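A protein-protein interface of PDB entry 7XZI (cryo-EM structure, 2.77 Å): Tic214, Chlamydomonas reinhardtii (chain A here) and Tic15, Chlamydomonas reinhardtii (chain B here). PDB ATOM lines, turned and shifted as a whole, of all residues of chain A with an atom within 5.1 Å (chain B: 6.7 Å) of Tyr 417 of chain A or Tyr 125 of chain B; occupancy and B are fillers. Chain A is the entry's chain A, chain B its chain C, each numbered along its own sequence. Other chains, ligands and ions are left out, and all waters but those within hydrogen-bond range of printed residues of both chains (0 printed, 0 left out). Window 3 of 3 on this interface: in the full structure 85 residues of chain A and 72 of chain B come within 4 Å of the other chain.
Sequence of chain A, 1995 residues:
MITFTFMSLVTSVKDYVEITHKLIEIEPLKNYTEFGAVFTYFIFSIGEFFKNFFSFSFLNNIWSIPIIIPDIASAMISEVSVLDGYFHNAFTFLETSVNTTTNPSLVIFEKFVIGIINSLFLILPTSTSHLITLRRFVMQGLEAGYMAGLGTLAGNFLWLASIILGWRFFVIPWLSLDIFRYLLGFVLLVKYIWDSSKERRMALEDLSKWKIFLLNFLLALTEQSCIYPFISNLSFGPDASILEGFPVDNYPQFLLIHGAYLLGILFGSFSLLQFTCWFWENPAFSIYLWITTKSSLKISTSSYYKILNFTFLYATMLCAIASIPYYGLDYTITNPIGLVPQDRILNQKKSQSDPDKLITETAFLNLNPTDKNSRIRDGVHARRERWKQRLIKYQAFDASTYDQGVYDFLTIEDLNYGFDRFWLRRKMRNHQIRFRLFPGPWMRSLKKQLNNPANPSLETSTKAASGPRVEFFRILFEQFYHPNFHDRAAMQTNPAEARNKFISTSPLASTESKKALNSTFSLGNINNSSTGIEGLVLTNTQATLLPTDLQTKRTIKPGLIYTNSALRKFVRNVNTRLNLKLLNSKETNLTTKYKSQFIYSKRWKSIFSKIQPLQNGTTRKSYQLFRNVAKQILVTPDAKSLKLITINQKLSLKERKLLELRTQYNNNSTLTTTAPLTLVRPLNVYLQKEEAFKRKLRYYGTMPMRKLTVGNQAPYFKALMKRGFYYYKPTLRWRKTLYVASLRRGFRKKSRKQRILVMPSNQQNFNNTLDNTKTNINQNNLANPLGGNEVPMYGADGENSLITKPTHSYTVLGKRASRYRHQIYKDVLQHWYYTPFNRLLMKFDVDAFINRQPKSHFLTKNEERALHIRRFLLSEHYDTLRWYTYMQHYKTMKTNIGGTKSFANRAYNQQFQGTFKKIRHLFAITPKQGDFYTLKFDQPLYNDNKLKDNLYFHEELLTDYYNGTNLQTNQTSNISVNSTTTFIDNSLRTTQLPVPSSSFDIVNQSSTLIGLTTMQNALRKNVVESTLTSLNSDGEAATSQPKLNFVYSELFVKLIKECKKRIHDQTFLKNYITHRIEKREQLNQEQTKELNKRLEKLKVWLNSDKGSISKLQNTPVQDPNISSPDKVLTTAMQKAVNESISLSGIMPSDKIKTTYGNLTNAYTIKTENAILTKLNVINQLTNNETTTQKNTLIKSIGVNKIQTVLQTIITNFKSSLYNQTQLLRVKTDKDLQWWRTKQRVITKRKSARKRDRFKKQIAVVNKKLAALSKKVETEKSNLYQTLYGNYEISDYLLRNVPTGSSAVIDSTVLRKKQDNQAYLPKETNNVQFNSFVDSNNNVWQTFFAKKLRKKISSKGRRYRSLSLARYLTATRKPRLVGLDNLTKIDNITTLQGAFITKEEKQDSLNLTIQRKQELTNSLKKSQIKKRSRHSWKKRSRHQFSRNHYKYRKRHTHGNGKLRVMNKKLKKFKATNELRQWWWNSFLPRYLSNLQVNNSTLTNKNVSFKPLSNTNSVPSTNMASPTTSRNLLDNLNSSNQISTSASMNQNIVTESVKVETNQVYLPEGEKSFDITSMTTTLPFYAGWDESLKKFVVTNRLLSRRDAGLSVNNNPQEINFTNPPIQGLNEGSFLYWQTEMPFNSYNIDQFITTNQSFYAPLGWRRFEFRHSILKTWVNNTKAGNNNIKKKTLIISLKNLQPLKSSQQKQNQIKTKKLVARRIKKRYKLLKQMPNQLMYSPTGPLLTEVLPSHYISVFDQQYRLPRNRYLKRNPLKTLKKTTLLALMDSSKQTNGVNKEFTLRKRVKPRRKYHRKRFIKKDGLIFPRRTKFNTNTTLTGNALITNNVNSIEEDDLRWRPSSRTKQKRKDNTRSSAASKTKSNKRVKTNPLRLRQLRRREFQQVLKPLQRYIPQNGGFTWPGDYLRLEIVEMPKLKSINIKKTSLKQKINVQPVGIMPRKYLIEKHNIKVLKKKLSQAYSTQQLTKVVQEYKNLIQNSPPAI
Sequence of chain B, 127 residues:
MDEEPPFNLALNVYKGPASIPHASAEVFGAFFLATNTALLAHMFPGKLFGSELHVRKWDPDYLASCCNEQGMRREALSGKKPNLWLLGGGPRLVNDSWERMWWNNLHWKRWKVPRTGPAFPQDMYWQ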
ATOM      1  N   ILE A 412       0.827   0.622   0.308  1.00  0.00           N
ATOM      2  CA  ILE A 412       0.571  -0.093  -0.938  1.00  0.00           C
ATOM      3  C   ILE A 412      -0.913  -0.411  -1.077  1.00  0.00           C
ATOM      4  O   ILE A 412      -1.488  -0.297  -2.166  1.00  0.00           O
ATOM      5  CB  ILE A 412       1.434  -1.366  -1.006  1.00  0.00           C
ATOM      6  CG1 ILE A 412       2.908  -1.020  -0.791  1.00  0.00           C
ATOM      7  CG2 ILE A 412       1.246  -2.070  -2.337  1.00  0.00           C
ATOM      8  CD1 ILE A 412       3.829  -2.220  -0.816  1.00  0.00           C
ATOM      9  N   GLU A 413      -1.553  -0.821   0.021  1.00  0.00           N
ATOM     10  CA  GLU A 413      -2.965  -1.186  -0.031  1.00  0.00           C
ATOM     11  C   GLU A 413      -3.838   0.006  -0.404  1.00  0.00           C
ATOM     12  O   GLU A 413      -4.793  -0.133  -1.176  1.00  0.00           O
ATOM     13  CB  GLU A 413      -3.407  -1.772   1.312  1.00  0.00           C
ATOM     14  CG  GLU A 413      -2.875  -3.172   1.596  1.00  0.00           C
ATOM     15  CD  GLU A 413      -1.414  -3.183   2.005  1.00  0.00           C
ATOM     16  OE1 GLU A 413      -0.842  -2.094   2.217  1.00  0.00           O
ATOM     17  OE2 GLU A 413      -0.835  -4.283   2.115  1.00  0.00           O
ATOM     18  N   ASP A 414      -3.533   1.186   0.142  1.00  0.00           N
ATOM     19  CA  ASP A 414      -4.308   2.375  -0.198  1.00  0.00           C
ATOM     20  C   ASP A 414      -4.151   2.738  -1.669  1.00  0.00           C
ATOM     21  O   ASP A 414      -5.114   3.166  -2.315  1.00  0.00           O
ATOM     22  CB  ASP A 414      -3.894   3.550   0.689  1.00  0.00           C
ATOM     23  CG  ASP A 414      -4.383   3.405   2.118  1.00  0.00           C
ATOM     24  OD1 ASP A 414      -5.475   2.834   2.321  1.00  0.00           O
ATOM     25  OD2 ASP A 414      -3.677   3.866   3.039  1.00  0.00           O
ATOM     26  N   LEU A 415      -2.946   2.580  -2.216  1.00  0.00           N
ATOM     27  CA  LEU A 415      -2.706   2.993  -3.594  1.00  0.00           C
ATOM     28  C   LEU A 415      -3.183   1.946  -4.596  1.00  0.00           C
ATOM     29  O   LEU A 415      -3.808   2.289  -5.606  1.00  0.00           O
ATOM     30  CB  LEU A 415      -1.220   3.294  -3.800  1.00  0.00           C
ATOM     31  CG  LEU A 415      -0.627   4.443  -2.980  1.00  0.00           C
ATOM     32  CD1 LEU A 415       0.857   4.603  -3.266  1.00  0.00           C
ATOM     33  CD2 LEU A 415      -1.368   5.740  -3.258  1.00  0.00           C
ATOM     34  N   ASN A 416      -2.909   0.667  -4.337  1.00  0.00           N
ATOM     35  CA  ASN A 416      -3.062  -0.359  -5.361  1.00  0.00           C
ATOM     36  C   ASN A 416      -4.116  -1.419  -5.058  1.00  0.00           C
ATOM     37  O   ASN A 416      -4.578  -2.081  -5.993  1.00  0.00           O
ATOM     38  CB  ASN A 416      -1.718  -1.056  -5.604  1.00  0.00           C
ATOM     39  CG  ASN A 416      -0.642  -0.098  -6.058  1.00  0.00           C
ATOM     40  OD1 ASN A 416       0.363   0.094  -5.376  1.00  0.00           O
ATOM     41  ND2 ASN A 416      -0.848   0.516  -7.218  1.00  0.00           N
ATOM     42  N   TYR A 417      -4.514  -1.611  -3.802  1.00  0.00           N
ATOM     43  CA  TYR A 417      -5.272  -2.804  -3.446  1.00  0.00           C
ATOM     44  C   TYR A 417      -6.721  -2.492  -3.107  1.00  0.00           C
ATOM     45  O   TYR A 417      -7.010  -1.564  -2.345  1.00  0.00           O
ATOM     46  CB  TYR A 417      -4.648  -3.549  -2.263  1.00  0.00           C
ATOM     47  CG  TYR A 417      -5.423  -4.794  -1.889  1.00  0.00           C
ATOM     48  CD1 TYR A 417      -5.392  -5.920  -2.699  1.00  0.00           C
ATOM     49  CD2 TYR A 417      -6.195  -4.840  -0.736  1.00  0.00           C
ATOM     50  CE1 TYR A 417      -6.099  -7.057  -2.370  1.00  0.00           C
ATOM     51  CE2 TYR A 417      -6.907  -5.977  -0.399  1.00  0.00           C
ATOM     52  CZ  TYR A 417      -6.853  -7.082  -1.220  1.00  0.00           C
ATOM     53  OH  TYR A 417      -7.556  -8.218  -0.896  1.00  0.00           O
ATOM     54  N   GLY A 418      -7.620  -3.284  -3.690  1.00  0.00           N
ATOM     55  CA  GLY A 418      -8.993  -3.445  -3.246  1.00  0.00           C
ATOM     56  C   GLY A 418      -9.812  -2.209  -2.942  1.00  0.00           C
ATOM     57  O   GLY A 418      -9.706  -1.185  -3.623  1.00  0.00           O
ATOM     58  N   PHE A 419     -10.642  -2.310  -1.901  1.00  0.00           N
ATOM     59  CA  PHE A 419     -11.609  -1.264  -1.593  1.00  0.00           C
ATOM     60  C   PHE A 419     -10.955  -0.008  -1.037  1.00  0.00           C
ATOM     61  O   PHE A 419     -11.556   1.068  -1.104  1.00  0.00           O
ATOM     62  CB  PHE A 419     -12.647  -1.800  -0.604  1.00  0.00           C
ATOM     63  CG  PHE A 419     -13.834  -0.902  -0.419  1.00  0.00           C
ATOM     64  CD1 PHE A 419     -14.837  -0.854  -1.372  1.00  0.00           C
ATOM     65  CD2 PHE A 419     -13.954  -0.119   0.714  1.00  0.00           C
ATOM     66  CE1 PHE A 419     -15.932  -0.034  -1.201  1.00  0.00           C
ATOM     67  CE2 PHE A 419     -15.048   0.702   0.890  1.00  0.00           C
ATOM     68  CZ  PHE A 419     -16.037   0.745  -0.068  1.00  0.00           C
ATOM     69  N   ASP A 420      -9.743  -0.116  -0.490  1.00  0.00           N
ATOM     70  CA  ASP A 420      -9.049   1.071   0.001  1.00  0.00           C
ATOM     71  C   ASP A 420      -8.788   2.050  -1.136  1.00  0.00           C
ATOM     72  O   ASP A 420      -9.102   3.242  -1.035  1.00  0.00           O
ATOM     73  CB  ASP A 420      -7.740   0.667   0.680  1.00  0.00           C
ATOM     74  CG  ASP A 420      -7.933  -0.427   1.712  1.00  0.00           C
ATOM     75  OD1 ASP A 420      -8.267  -1.564   1.317  1.00  0.00           O
ATOM     76  OD2 ASP A 420      -7.754  -0.150   2.916  1.00  0.00           O
ATOM     77  N   ARG A 421      -8.224   1.552  -2.238  1.00  0.00           N
ATOM     78  CA  ARG A 421      -8.047   2.374  -3.429  1.00  0.00           C
ATOM     79  C   ARG A 421      -9.387   2.835  -3.985  1.00  0.00           C
ATOM     80  O   ARG A 421      -9.529   3.989  -4.404  1.00  0.00           O
ATOM     81  CB  ARG A 421      -7.268   1.586  -4.481  1.00  0.00           C
ATOM     82  CG  ARG A 421      -7.215   2.232  -5.849  1.00  0.00           C
ATOM     83  CD  ARG A 421      -6.836   1.211  -6.908  1.00  0.00           C
ATOM     84  NE  ARG A 421      -6.836   1.787  -8.244  1.00  0.00           N
ATOM     85  CZ  ARG A 421      -7.925   1.963  -8.984  1.00  0.00           C
ATOM     86  NH1 ARG A 421      -9.126   1.628  -8.538  1.00  0.00           N
ATOM     87  NH2 ARG A 421      -7.806   2.492 -10.197  1.00  0.00           N
ATOM     88  N   TYR A 834     -17.055  -7.129  -2.330  1.00  0.00           N
ATOM     89  CA  TYR A 834     -16.463  -8.450  -2.501  1.00  0.00           C
ATOM     90  C   TYR A 834     -17.509  -9.553  -2.618  1.00  0.00           C
ATOM     91  O   TYR A 834     -17.200 -10.722  -2.361  1.00  0.00           O
ATOM     92  CB  TYR A 834     -15.506  -8.758  -1.350  1.00  0.00           C
ATOM     93  CG  TYR A 834     -14.272  -7.891  -1.328  1.00  0.00           C
ATOM     94  CD1 TYR A 834     -13.244  -8.092  -2.238  1.00  0.00           C
ATOM     95  CD2 TYR A 834     -14.128  -6.879  -0.392  1.00  0.00           C
ATOM     96  CE1 TYR A 834     -12.114  -7.306  -2.221  1.00  0.00           C
ATOM     97  CE2 TYR A 834     -12.998  -6.088  -0.367  1.00  0.00           C
ATOM     98  CZ  TYR A 834     -11.996  -6.306  -1.285  1.00  0.00           C
ATOM     99  OH  TYR A 834     -10.866  -5.522  -1.267  1.00  0.00           O
ATOM    100  N   LEU A 922      -8.652  -8.204   7.442  1.00  0.00           N
ATOM    101  CA  LEU A 922      -8.894  -8.962   6.220  1.00  0.00           C
ATOM    102  C   LEU A 922      -8.431 -10.411   6.305  1.00  0.00           C
ATOM    103  O   LEU A 922      -9.207 -11.319   5.996  1.00  0.00           O
ATOM    104  CB  LEU A 922      -8.209  -8.278   5.033  1.00  0.00           C
ATOM    105  CG  LEU A 922      -8.713  -6.876   4.690  1.00  0.00           C
ATOM    106  CD1 LEU A 922      -7.976  -6.314   3.486  1.00  0.00           C
ATOM    107  CD2 LEU A 922     -10.212  -6.899   4.442  1.00  0.00           C
ATOM    108  N   PHE A 923      -7.189 -10.654   6.716  1.00  0.00           N
ATOM    109  CA  PHE A 923      -6.630 -11.999   6.753  1.00  0.00           C
ATOM    110  C   PHE A 923      -6.156 -12.319   8.166  1.00  0.00           C
ATOM    111  O   PHE A 923      -6.198 -11.480   9.070  1.00  0.00           O
ATOM    112  CB  PHE A 923      -5.479 -12.151   5.751  1.00  0.00           C
ATOM    113  CG  PHE A 923      -5.861 -11.843   4.332  1.00  0.00           C
ATOM    114  CD1 PHE A 923      -6.681 -12.701   3.619  1.00  0.00           C
ATOM    115  CD2 PHE A 923      -5.389 -10.701   3.707  1.00  0.00           C
ATOM    116  CE1 PHE A 923      -7.031 -12.420   2.313  1.00  0.00           C
ATOM    117  CE2 PHE A 923      -5.735 -10.416   2.401  1.00  0.00           C
ATOM    118  CZ  PHE A 923      -6.556 -11.276   1.703  1.00  0.00           C
ATOM    119  N   MET B  43      -1.335  -8.083 -21.254  1.00  0.00           N
ATOM    120  CA  MET B  43      -1.962  -8.237 -19.943  1.00  0.00           C
ATOM    121  C   MET B  43      -1.996  -9.695 -19.497  1.00  0.00           C
ATOM    122  O   MET B  43      -1.737  -9.995 -18.326  1.00  0.00           O
ATOM    123  CB  MET B  43      -3.374  -7.654 -19.958  1.00  0.00           C
ATOM    124  CG  MET B  43      -3.420  -6.140 -20.032  1.00  0.00           C
ATOM    125  SD  MET B  43      -5.065  -5.479 -19.712  1.00  0.00           S
ATOM    126  CE  MET B  43      -5.333  -6.047 -18.036  1.00  0.00           C
ATOM    127  N   ASP B 123       2.349 -10.188 -13.899  1.00  0.00           N
ATOM    128  CA  ASP B 123       1.197 -11.020 -13.601  1.00  0.00           C
ATOM    129  C   ASP B 123      -0.079 -10.183 -13.686  1.00  0.00           C
ATOM    130  O   ASP B 123      -0.056  -9.009 -14.066  1.00  0.00           O
ATOM    131  CB  ASP B 123       1.366 -11.678 -12.229  1.00  0.00           C
ATOM    132  CG  ASP B 123       0.618 -12.992 -12.122  1.00  0.00           C
ATOM    133  OD1 ASP B 123       0.114 -13.474 -13.158  1.00  0.00           O
ATOM    134  OD2 ASP B 123       0.530 -13.542 -11.004  1.00  0.00           O
ATOM    135  N   MET B 124      -1.209 -10.788 -13.329  1.00  0.00           N
ATOM    136  CA  MET B 124      -2.512 -10.148 -13.431  1.00  0.00           C
ATOM    137  C   MET B 124      -3.111  -9.967 -12.045  1.00  0.00           C
ATOM    138  O   MET B 124      -3.116 -10.903 -11.238  1.00  0.00           O
ATOM    139  CB  MET B 124      -3.462 -10.960 -14.314  1.00  0.00           C
ATOM    140  CG  MET B 124      -4.838 -10.336 -14.470  1.00  0.00           C
ATOM    141  SD  MET B 124      -4.770  -8.664 -15.139  1.00  0.00           S
ATOM    142  CE  MET B 124      -6.507  -8.228 -15.145  1.00  0.00           C
ATOM    143  N   TYR B 125      -3.617  -8.768 -11.778  1.00  0.00           N
ATOM    144  CA  TYR B 125      -4.260  -8.428 -10.520  1.00  0.00           C
ATOM    145  C   TYR B 125      -5.722  -8.084 -10.776  1.00  0.00           C
ATOM    146  O   TYR B 125      -6.093  -7.689 -11.886  1.00  0.00           O
ATOM    147  CB  TYR B 125      -3.540  -7.258  -9.830  1.00  0.00           C
ATOM    148  CG  TYR B 125      -4.354  -6.555  -8.769  1.00  0.00           C
ATOM    149  CD1 TYR B 125      -4.680  -7.194  -7.581  1.00  0.00           C
ATOM    150  CD2 TYR B 125      -4.795  -5.253  -8.955  1.00  0.00           C
ATOM    151  CE1 TYR B 125      -5.424  -6.557  -6.610  1.00  0.00           C
ATOM    152  CE2 TYR B 125      -5.540  -4.608  -7.988  1.00  0.00           C
ATOM    153  CZ  TYR B 125      -5.850  -5.265  -6.818  1.00  0.00           C
ATOM    154  OH  TYR B 125      -6.593  -4.626  -5.852  1.00  0.00           O
ATOM    155  N   TRP B 126      -6.551  -8.291  -9.748  1.00  0.00           N
ATOM    156  CA  TRP B 126      -7.981  -7.990  -9.762  1.00  0.00           C
ATOM    157  C   TRP B 126      -8.746  -9.005 -10.602  1.00  0.00           C
ATOM    158  O   TRP B 126      -9.977  -8.961 -10.670  1.00  0.00           O
ATOM    159  CB  TRP B 126      -8.244  -6.568 -10.267  1.00  0.00           C
ATOM    160  CG  TRP B 126      -8.844  -5.665  -9.243  1.00  0.00           C
ATOM    161  CD1 TRP B 126      -9.445  -6.034  -8.076  1.00  0.00           C
ATOM    162  CD2 TRP B 126      -8.896  -4.234  -9.287  1.00  0.00           C
ATOM    163  NE1 TRP B 126      -9.871  -4.922  -7.392  1.00  0.00           N
ATOM    164  CE2 TRP B 126      -9.547  -3.805  -8.114  1.00  0.00           C
ATOM    165  CE3 TRP B 126      -8.457  -3.274 -10.205  1.00  0.00           C
ATOM    166  CZ2 TRP B 126      -9.768  -2.459  -7.833  1.00  0.00           C
ATOM    167  CZ3 TRP B 126      -8.678  -1.940  -9.925  1.00  0.00           C
ATOM    168  CH2 TRP B 126      -9.328  -1.545  -8.749  1.00  0.00           C
ATOM    169  N   GLN B 127      -8.024  -9.925 -11.235  1.00  0.00           N
ATOM    170  CA  GLN B 127      -8.632 -11.002 -12.005  1.00  0.00           C
ATOM    171  C   GLN B 127      -7.754 -12.245 -11.931  1.00  0.00           C
ATOM    172  O   GLN B 127      -6.553 -12.153 -11.676  1.00  0.00           O
ATOM    173  CB  GLN B 127      -8.851 -10.591 -13.466  1.00  0.00           C
ATOM    174  CG  GLN B 127     -10.099  -9.754 -13.715  1.00  0.00           C
ATOM    175  CD  GLN B 127     -10.413  -9.587 -15.192  1.00  0.00           C
ATOM    176  OE1 GLN B 127      -9.799 -10.224 -16.046  1.00  0.00           O
ATOM    177  NE2 GLN B 127     -11.377  -8.726 -15.498  1.00  0.00           N
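Tyr 125 of chain B touches Tyr 417 of chain A. Arg 421 of chain A touches Trp 126 of chain B.
Hydrophobic or aromatic side chains of chain A that line the printed part of chain B: Tyr 417. Among the printed residues, no Asp or Glu carboxylate lies within 4 Å of a Lys or Arg side-chain nitrogen of the other chain.
The backbone carbonyl oxygen (O) of Asn 416 of chain A lies within hydrogen-bond range of the side-chain hydroxyl (OH) of Tyr 125 of chain B (3.2 Å). OH of Tyr 125 of chain B is in hydrogen-bond range of N of Gly 418 of chain A (2.7 Å).
Tyr 417 of chain A touches just one residue of chain B: Tyr 125 (3.3 Å). Tyr 125 of chain B touches three residues of chain A. Of the printed residues of chain B, Gly 418 of chain A touches Tyr 125. Printed residues of chain A within 4 Å of Trp 126 of chain B: Arg 421 (3.2 Å). Leu 922 of chain A touches none of the printed residues of chain B. Tyr 834 of chain A touches none of the printed residues of chain B. The nearest residue of chain B that does not touch Tyr 417 of chain A is Trp 126 of chain B (5.6 Å). The nearest printed residue of chain A that does not touch Tyr 125 of chain B is Arg 421 of chain A (5.9 Å).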
